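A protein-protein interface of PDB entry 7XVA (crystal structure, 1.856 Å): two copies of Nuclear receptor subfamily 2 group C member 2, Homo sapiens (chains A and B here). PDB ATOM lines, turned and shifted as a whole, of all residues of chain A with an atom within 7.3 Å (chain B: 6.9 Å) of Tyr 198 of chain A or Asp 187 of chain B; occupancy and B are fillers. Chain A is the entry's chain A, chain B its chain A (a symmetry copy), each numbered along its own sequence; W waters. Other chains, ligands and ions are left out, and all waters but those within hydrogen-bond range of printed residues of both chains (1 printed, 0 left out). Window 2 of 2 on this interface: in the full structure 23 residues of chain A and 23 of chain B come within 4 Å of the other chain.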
ATOM      1  N   VAL A 189      19.344  -9.568  -0.247  1.00  0.00           N
ATOM      2  CA  VAL A 189      18.079 -10.242  -0.663  1.00  0.00           C
ATOM      3  C   VAL A 189      16.922  -9.252  -0.412  1.00  0.00           C
ATOM      4  O   VAL A 189      16.059  -9.168  -1.272  1.00  0.00           O
ATOM      5  CB  VAL A 189      17.876 -11.593   0.061  1.00  0.00           C
ATOM      6  CG1 VAL A 189      16.494 -12.168  -0.198  1.00  0.00           C
ATOM      7  CG2 VAL A 189      18.956 -12.590  -0.353  1.00  0.00           C
ATOM      8  N   TYR A 193      15.110  -8.374  -3.827  1.00  0.00           N
ATOM      9  CA  TYR A 193      13.940  -9.281  -3.987  1.00  0.00           C
ATOM     10  C   TYR A 193      12.915  -8.921  -2.907  1.00  0.00           C
ATOM     11  O   TYR A 193      12.446  -9.827  -2.185  1.00  0.00           O
ATOM     12  CB  TYR A 193      14.385 -10.751  -3.943  1.00  0.00           C
ATOM     13  CG  TYR A 193      15.386 -11.166  -4.994  1.00  0.00           C
ATOM     14  CD1 TYR A 193      15.001 -11.347  -6.313  1.00  0.00           C
ATOM     15  CD2 TYR A 193      16.723 -11.402  -4.679  1.00  0.00           C
ATOM     16  CE1 TYR A 193      15.906 -11.724  -7.292  1.00  0.00           C
ATOM     17  CE2 TYR A 193      17.639 -11.801  -5.645  1.00  0.00           C
ATOM     18  CZ  TYR A 193      17.228 -11.960  -6.960  1.00  0.00           C
ATOM     19  OH  TYR A 193      18.104 -12.321  -7.951  1.00  0.00           O
ATOM     20  N   SER A 194      12.565  -7.628  -2.818  1.00  0.00           N
ATOM     21  CA  SER A 194      11.733  -7.043  -1.732  1.00  0.00           C
ATOM     22  C   SER A 194      10.344  -7.699  -1.699  1.00  0.00           C
ATOM     23  O   SER A 194       9.791  -7.837  -0.595  1.00  0.00           O
ATOM     24  CB  SER A 194      11.630  -5.539  -1.873  1.00  0.00           C
ATOM     25  OG  SER A 194      11.142  -5.207  -3.168  1.00  0.00           O
ATOM     26  N   GLU A 195       9.817  -8.107  -2.851  1.00  0.00           N
ATOM     27  CA  GLU A 195       8.456  -8.690  -2.984  1.00  0.00           C
ATOM     28  C   GLU A 195       8.472 -10.182  -2.617  1.00  0.00           C
ATOM     29  O   GLU A 195       7.375 -10.746  -2.476  1.00  0.00           O
ATOM     30  CB  GLU A 195       7.940  -8.533  -4.415  1.00  0.00           C
ATOM     31  N   ASP A 196       9.658 -10.809  -2.533  1.00  0.00           N
ATOM     32  CA  ASP A 196       9.826 -12.254  -2.215  1.00  0.00           C
ATOM     33  C   ASP A 196      10.243 -12.324  -0.744  1.00  0.00           C
ATOM     34  O   ASP A 196      11.440 -12.458  -0.439  1.00  0.00           O
ATOM     35  CB  ASP A 196      10.787 -12.890  -3.219  1.00  0.00           C
ATOM     36  CG  ASP A 196      10.809 -14.408  -3.236  1.00  0.00           C
ATOM     37  OD1 ASP A 196      10.182 -15.025  -2.334  1.00  0.00           O
ATOM     38  OD2 ASP A 196      11.494 -14.966  -4.151  1.00  0.00           O
ATOM     39  N   THR A 197       9.260 -12.164   0.131  1.00  0.00           N
ATOM     40  CA  THR A 197       9.388 -12.033   1.599  1.00  0.00           C
ATOM     41  C   THR A 197      10.224 -13.177   2.172  1.00  0.00           C
ATOM     42  O   THR A 197      10.918 -12.962   3.166  1.00  0.00           O
ATOM     43  CB  THR A 197       8.008 -12.156   2.266  1.00  0.00           C
ATOM     44  OG1 THR A 197       7.090 -11.532   1.368  1.00  0.00           O
ATOM     45  CG2 THR A 197       7.983 -11.550   3.647  1.00  0.00           C
ATOM     46  N   TYR A 198      10.087 -14.357   1.600  1.00  0.00           N
ATOM     47  CA  TYR A 198      10.576 -15.619   2.232  1.00  0.00           C
ATOM     48  C   TYR A 198      11.845 -16.135   1.550  1.00  0.00           C
ATOM     49  O   TYR A 198      12.332 -17.216   1.933  1.00  0.00           O
ATOM     50  CB  TYR A 198       9.470 -16.668   2.259  1.00  0.00           C
ATOM     51  CG  TYR A 198       8.329 -16.277   3.163  1.00  0.00           C
ATOM     52  CD1 TYR A 198       8.494 -16.215   4.526  1.00  0.00           C
ATOM     53  CD2 TYR A 198       7.097 -15.895   2.640  1.00  0.00           C
ATOM     54  CE1 TYR A 198       7.461 -15.848   5.364  1.00  0.00           C
ATOM     55  CE2 TYR A 198       6.056 -15.500   3.459  1.00  0.00           C
ATOM     56  CZ  TYR A 198       6.241 -15.460   4.828  1.00  0.00           C
ATOM     57  OH  TYR A 198       5.228 -15.066   5.666  1.00  0.00           O
ATOM     58  N   ARG A 199      12.426 -15.364   0.649  1.00  0.00           N
ATOM     59  CA  ARG A 199      13.524 -15.860  -0.219  1.00  0.00           C
ATOM     60  C   ARG A 199      14.756 -16.237   0.630  1.00  0.00           C
ATOM     61  O   ARG A 199      15.396 -17.294   0.332  1.00  0.00           O
ATOM     62  CB  ARG A 199      13.958 -14.817  -1.241  1.00  0.00           C
ATOM     63  CG  ARG A 199      14.999 -15.363  -2.211  1.00  0.00           C
ATOM     64  CD  ARG A 199      15.284 -14.439  -3.361  1.00  0.00           C
ATOM     65  NE  ARG A 199      16.371 -14.912  -4.216  1.00  0.00           N
ATOM     66  CZ  ARG A 199      16.262 -15.867  -5.114  1.00  0.00           C
ATOM     67  NH1 ARG A 199      15.126 -16.546  -5.242  1.00  0.00           N
ATOM     68  NH2 ARG A 199      17.291 -16.177  -5.875  1.00  0.00           N
ATOM     69  N   LEU A 200      15.147 -15.376   1.559  1.00  0.00           N
ATOM     70  CA  LEU A 200      16.397 -15.588   2.340  1.00  0.00           C
ATOM     71  C   LEU A 200      16.297 -16.938   3.067  1.00  0.00           C
ATOM     72  O   LEU A 200      17.261 -17.734   2.974  1.00  0.00           O
ATOM     73  CB  LEU A 200      16.623 -14.472   3.352  1.00  0.00           C
ATOM     74  CG  LEU A 200      17.834 -14.702   4.253  1.00  0.00           C
ATOM     75  CD1 LEU A 200      19.117 -14.589   3.456  1.00  0.00           C
ATOM     76  CD2 LEU A 200      17.827 -13.749   5.426  1.00  0.00           C
ATOM     77  N   ALA A 201      15.178 -17.184   3.747  1.00  0.00           N
ATOM     78  CA  ALA A 201      14.940 -18.437   4.494  1.00  0.00           C
ATOM     79  C   ALA A 201      15.056 -19.617   3.519  1.00  0.00           C
ATOM     80  O   ALA A 201      15.723 -20.626   3.883  1.00  0.00           O
ATOM     81  CB  ALA A 201      13.601 -18.409   5.189  1.00  0.00           C
ATOM     82  N   ARG A 202      14.466 -19.491   2.321  1.00  0.00           N
ATOM     83  CA  ARG A 202      14.478 -20.562   1.294  1.00  0.00           C
ATOM     84  C   ARG A 202      15.916 -20.890   0.914  1.00  0.00           C
ATOM     85  O   ARG A 202      16.249 -22.068   0.790  1.00  0.00           O
ATOM     86  CB  ARG A 202      13.769 -20.159  -0.002  1.00  0.00           C
ATOM     87  CG  ARG A 202      12.280 -20.433   0.022  1.00  0.00           C
ATOM     88  CD  ARG A 202      11.627 -20.224  -1.334  1.00  0.00           C
ATOM     89  NE  ARG A 202      10.268 -19.787  -1.059  1.00  0.00           N
ATOM     90  CZ  ARG A 202       9.840 -18.535  -1.168  1.00  0.00           C
ATOM     91  NH1 ARG A 202      10.645 -17.598  -1.639  1.00  0.00           N
ATOM     92  NH2 ARG A 202       8.583 -18.246  -0.866  1.00  0.00           N
ATOM     93  N   ILE A 203      16.731 -19.867   0.702  1.00  0.00           N
ATOM     94  CA  ILE A 203      18.140 -20.064   0.276  1.00  0.00           C
ATOM     95  C   ILE A 203      18.939 -20.707   1.418  1.00  0.00           C
ATOM     96  O   ILE A 203      19.705 -21.637   1.140  1.00  0.00           O
ATOM     97  CB  ILE A 203      18.766 -18.738  -0.182  1.00  0.00           C
ATOM     98  CG1 ILE A 203      18.084 -18.176  -1.428  1.00  0.00           C
ATOM     99  CG2 ILE A 203      20.238 -18.933  -0.412  1.00  0.00           C
ATOM    100  CD1 ILE A 203      18.376 -16.677  -1.603  1.00  0.00           C
ATOM    101  N   LEU A 204      18.832 -20.206   2.649  1.00  0.00           N
ATOM    102  CA  LEU A 204      19.668 -20.742   3.747  1.00  0.00           C
ATOM    103  C   LEU A 204      19.334 -22.208   4.051  1.00  0.00           C
ATOM    104  O   LEU A 204      20.244 -22.972   4.455  1.00  0.00           O
ATOM    105  CB  LEU A 204      19.484 -19.867   4.978  1.00  0.00           C
ATOM    106  CG  LEU A 204      20.020 -18.454   4.815  1.00  0.00           C
ATOM    107  CD1 LEU A 204      19.726 -17.657   6.066  1.00  0.00           C
ATOM    108  CD2 LEU A 204      21.514 -18.495   4.522  1.00  0.00           C
ATOM    109  N   GLU B 179       8.681 -25.916   3.349  1.00  0.00           N
ATOM    110  CA  GLU B 179       8.483 -24.480   3.007  1.00  0.00           C
ATOM    111  C   GLU B 179       7.539 -23.813   3.998  1.00  0.00           C
ATOM    112  O   GLU B 179       7.835 -22.694   4.372  1.00  0.00           O
ATOM    113  CB  GLU B 179       7.975 -24.298   1.571  1.00  0.00           C
ATOM    114  CG  GLU B 179       9.006 -24.651   0.517  1.00  0.00           C
ATOM    115  CD  GLU B 179       8.457 -24.893  -0.886  1.00  0.00           C
ATOM    116  OE1 GLU B 179       7.208 -24.755  -1.074  1.00  0.00           O
ATOM    117  OE2 GLU B 179       9.278 -25.227  -1.794  1.00  0.00           O
ATOM    118  N   GLN B 182       9.436 -23.089   7.331  1.00  0.00           N
ATOM    119  CA  GLN B 182      10.318 -21.916   7.093  1.00  0.00           C
ATOM    120  C   GLN B 182       9.503 -20.631   7.210  1.00  0.00           C
ATOM    121  O   GLN B 182       9.919 -19.722   7.914  1.00  0.00           O
ATOM    122  CB  GLN B 182      10.923 -21.942   5.699  1.00  0.00           C
ATOM    123  CG  GLN B 182      11.953 -23.022   5.501  1.00  0.00           C
ATOM    124  CD  GLN B 182      12.242 -23.233   4.041  1.00  0.00           C
ATOM    125  OE1 GLN B 182      12.297 -22.285   3.255  1.00  0.00           O
ATOM    126  NE2 GLN B 182      12.472 -24.480   3.678  1.00  0.00           N
ATOM    127  N   MET B 183       8.348 -20.577   6.553  1.00  0.00           N
ATOM    128  CA  MET B 183       7.504 -19.344   6.529  1.00  0.00           C
ATOM    129  C   MET B 183       6.958 -19.035   7.923  1.00  0.00           C
ATOM    130  O   MET B 183       7.071 -17.866   8.381  1.00  0.00           O
ATOM    131  CB  MET B 183       6.381 -19.505   5.504  1.00  0.00           C
ATOM    132  CG  MET B 183       6.931 -19.628   4.095  1.00  0.00           C
ATOM    133  SD  MET B 183       5.671 -19.892   2.795  1.00  0.00           S
ATOM    134  CE  MET B 183       4.463 -18.707   3.389  1.00  0.00           C
ATOM    135  N   GLU B 184       6.477 -20.063   8.621  1.00  0.00           N
ATOM    136  CA  GLU B 184       5.940 -19.942   9.990  1.00  0.00           C
ATOM    137  C   GLU B 184       7.065 -19.561  10.948  1.00  0.00           C
ATOM    138  O   GLU B 184       6.822 -18.684  11.796  1.00  0.00           O
ATOM    139  CB  GLU B 184       5.237 -21.244  10.389  1.00  0.00           C
ATOM    140  CG  GLU B 184       3.960 -21.455   9.604  1.00  0.00           C
ATOM    141  CD  GLU B 184       3.320 -22.824   9.732  1.00  0.00           C
ATOM    142  OE1 GLU B 184       3.437 -23.466  10.825  1.00  0.00           O
ATOM    143  OE2 GLU B 184       2.741 -23.271   8.718  1.00  0.00           O
ATOM    144  N   LEU B 185       8.267 -20.137  10.824  1.00  0.00           N
ATOM    145  CA  LEU B 185       9.388 -19.682  11.696  1.00  0.00           C
ATOM    146  C   LEU B 185       9.722 -18.198  11.454  1.00  0.00           C
ATOM    147  O   LEU B 185       9.922 -17.473  12.452  1.00  0.00           O
ATOM    148  CB  LEU B 185      10.608 -20.553  11.434  1.00  0.00           C
ATOM    149  CG  LEU B 185      11.868 -20.178  12.198  1.00  0.00           C
ATOM    150  CD1 LEU B 185      11.653 -20.150  13.692  1.00  0.00           C
ATOM    151  CD2 LEU B 185      12.968 -21.151  11.829  1.00  0.00           C
ATOM    152  N   GLN B 186       9.814 -17.746  10.205  1.00  0.00           N
ATOM    153  CA  GLN B 186      10.119 -16.312   9.902  1.00  0.00           C
ATOM    154  C   GLN B 186       9.049 -15.398  10.529  1.00  0.00           C
ATOM    155  O   GLN B 186       9.411 -14.448  11.255  1.00  0.00           O
ATOM    156  CB  GLN B 186      10.216 -16.086   8.398  1.00  0.00           C
ATOM    157  CG  GLN B 186      10.504 -14.638   8.018  1.00  0.00           C
ATOM    158  CD  GLN B 186      10.846 -14.485   6.556  1.00  0.00           C
ATOM    159  OE1 GLN B 186      11.464 -15.346   5.923  1.00  0.00           O
ATOM    160  NE2 GLN B 186      10.435 -13.369   5.976  1.00  0.00           N
ATOM    161  N   ASP B 187       7.764 -15.707  10.324  1.00  0.00           N
ATOM    162  CA  ASP B 187       6.647 -14.896  10.910  1.00  0.00           C
ATOM    163  C   ASP B 187       6.795 -14.825  12.423  1.00  0.00           C
ATOM    164  O   ASP B 187       6.659 -13.696  12.986  1.00  0.00           O
ATOM    165  CB  ASP B 187       5.273 -15.438  10.518  1.00  0.00           C
ATOM    166  CG  ASP B 187       5.001 -15.303   9.036  1.00  0.00           C
ATOM    167  OD1 ASP B 187       5.666 -14.464   8.395  1.00  0.00           O
ATOM    168  OD2 ASP B 187       4.157 -16.058   8.516  1.00  0.00           O
ATOM    169  N   TYR B 188       7.071 -15.953  13.094  1.00  0.00           N
ATOM    170  CA  TYR B 188       7.263 -15.983  14.557  1.00  0.00           C
ATOM    171  C   TYR B 188       8.460 -15.116  14.955  1.00  0.00           C
ATOM    172  O   TYR B 188       8.395 -14.412  15.983  1.00  0.00           O
ATOM    173  CB  TYR B 188       7.433 -17.417  15.076  1.00  0.00           C
ATOM    174  CG  TYR B 188       7.780 -17.455  16.536  1.00  0.00           C
ATOM    175  CD1 TYR B 188       6.795 -17.390  17.501  1.00  0.00           C
ATOM    176  CD2 TYR B 188       9.102 -17.450  16.950  1.00  0.00           C
ATOM    177  CE1 TYR B 188       7.111 -17.369  18.848  1.00  0.00           C
ATOM    178  CE2 TYR B 188       9.434 -17.427  18.290  1.00  0.00           C
ATOM    179  CZ  TYR B 188       8.432 -17.407  19.246  1.00  0.00           C
ATOM    180  OH  TYR B 188       8.754 -17.381  20.570  1.00  0.00           O
ATOM    181  N   VAL B 189       9.593 -15.238  14.243  1.00  0.00           N
ATOM    182  CA  VAL B 189      10.827 -14.510  14.659  1.00  0.00           C
ATOM    183  C   VAL B 189      10.575 -13.004  14.437  1.00  0.00           C
ATOM    184  O   VAL B 189      10.957 -12.237  15.306  1.00  0.00           O
ATOM    185  CB  VAL B 189      12.082 -15.022  13.914  1.00  0.00           C
ATOM    186  CG1 VAL B 189      13.290 -14.140  14.177  1.00  0.00           C
ATOM    187  CG2 VAL B 189      12.382 -16.468  14.300  1.00  0.00           C
ATOM    188  N   GLN B 190       9.947 -12.615  13.333  1.00  0.00           N
ATOM    189  CA  GLN B 190       9.638 -11.182  13.031  1.00  0.00           C
ATOM    190  C   GLN B 190       8.680 -10.600  14.088  1.00  0.00           C
ATOM    191  O   GLN B 190       8.950  -9.501  14.597  1.00  0.00           O
ATOM    192  CB  GLN B 190       9.091 -11.054  11.613  1.00  0.00           C
ATOM    193  CG  GLN B 190      10.169 -11.304  10.569  1.00  0.00           C
ATOM    194  CD  GLN B 190       9.673 -11.052   9.168  1.00  0.00           C
ATOM    195  OE1 GLN B 190       8.473 -10.906   8.937  1.00  0.00           O
ATOM    196  NE2 GLN B 190      10.598 -11.009   8.222  1.00  0.00           N
ATOM    197  N   LYS B 191       7.649 -11.346  14.481  1.00  0.00           N
ATOM    198  CA  LYS B 191       6.669 -10.890  15.501  1.00  0.00           C
ATOM    199  C   LYS B 191       7.312 -10.808  16.891  1.00  0.00           C
ATOM    200  O   LYS B 191       6.983  -9.878  17.629  1.00  0.00           O
ATOM    201  CB  LYS B 191       5.478 -11.842  15.513  1.00  0.00           C
ATOM    202  CG  LYS B 191       4.507 -11.665  16.665  1.00  0.00           C
ATOM    203  CD  LYS B 191       3.284 -12.551  16.524  1.00  0.00           C
ATOM    204  CE  LYS B 191       3.649 -14.015  16.385  1.00  0.00           C
ATOM    205  NZ  LYS B 191       2.454 -14.897  16.378  1.00  0.00           N
ATOM    206  N   THR B 192       8.155 -11.769  17.269  1.00  0.00           N
ATOM    207  CA  THR B 192       8.631 -11.964  18.664  1.00  0.00           C
ATOM    208  C   THR B 192       9.955 -11.241  18.915  1.00  0.00           C
ATOM    209  O   THR B 192      10.202 -10.890  20.088  1.00  0.00           O
ATOM    210  CB  THR B 192       8.806 -13.448  18.998  1.00  0.00           C
ATOM    211  OG1 THR B 192       7.646 -14.136  18.533  1.00  0.00           O
ATOM    212  CG2 THR B 192       8.997 -13.686  20.478  1.00  0.00           C
ATOM    213  N   LEU B 200      16.716 -14.612  12.378  1.00  0.00           N
ATOM    214  CA  LEU B 200      16.244 -15.779  11.582  1.00  0.00           C
ATOM    215  C   LEU B 200      17.445 -16.378  10.832  1.00  0.00           C
ATOM    216  O   LEU B 200      17.629 -17.616  10.903  1.00  0.00           O
ATOM    217  CB  LEU B 200      15.162 -15.379  10.587  1.00  0.00           C
ATOM    218  CG  LEU B 200      14.725 -16.519   9.670  1.00  0.00           C
ATOM    219  CD1 LEU B 200      13.973 -17.573  10.457  1.00  0.00           C
ATOM    220  CD2 LEU B 200      13.901 -16.001   8.514  1.00  0.00           C
HETATM  221  O   HOH W   1      13.328 -14.825   4.397  1.00  0.00           O
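The backbone carbonyl oxygen of Thr 197 of chain A sits at hydrogen-bond distance from the side-chain amide nitrogen of Gln 186 of chain B (2.9 Å). OD1 of Asp 187 of chain B sits at hydrogen-bond distance from OH of Tyr 198 of chain A (2.8 Å).
The side-chain carboxylate (OD1) of Asp 196 of chain A lies within salt-bridge range of the guanidinium group (NH1) of Arg 202 of chain A (2.7 Å). NE2 of Gln 186 of chain B sits close to NE2 of Gln 190 of chain B (3.3 Å).
Tyr 198 of chain A touches Met 183 of chain B (CE2 to CE, 3.6 Å). CD1 of Tyr 198 of chain A touches OE1 of Gln 186 of chain B, at 3.4 Å. Gln 182 of chain B touches Ala 201 of chain A. Ala 201 of chain A touches Gln 186 of chain B. Arg 202 of chain A touches Gln 182 of chain B (CA to OE1, 3.4 Å).
Of the printed residues of chain B, Ala 201 of chain A touches Gln 182 and Gln 186. Of the printed residues of chain A, Met 183 of chain B touches Tyr 198 (3.6 Å). Of chain A, only Tyr 198 (2.8 Å) comes within 4 Å of Asp 187 of chain B. The nearest residue of chain B that does not touch Tyr 198 of chain A is Gln 182 of chain B (5.1 Å). The nearest residue of chain A that does not touch Asp 187 of chain B is Thr 197 of chain A (6.0 Å). The nearest printed residue of chain B that does not touch Ala 201 of chain A is Leu 200 of chain B (4.1 Å).
Hydrophobic or aromatic side chains of chain B within 4 Å of the printed part of chain A: Met 183. Hydrophobic or aromatic side chains of chain A that line the printed part of chain B: Tyr 198 and Ala 201.
Positions printed for both chains: 189 and 200. Of the 7 pairs that touch across the chains among the printed residues, none has its exchanged pair printed and touching as well.
Water W1 lies within hydrogen-bond range of OE1 of Gln 186 of chain B (2.5 Å), N of Ala 201 of chain A (3.1 Å), O of Thr 197 of chain A (3.3 Å) and N of Leu 200 of chain A (3.4 Å).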
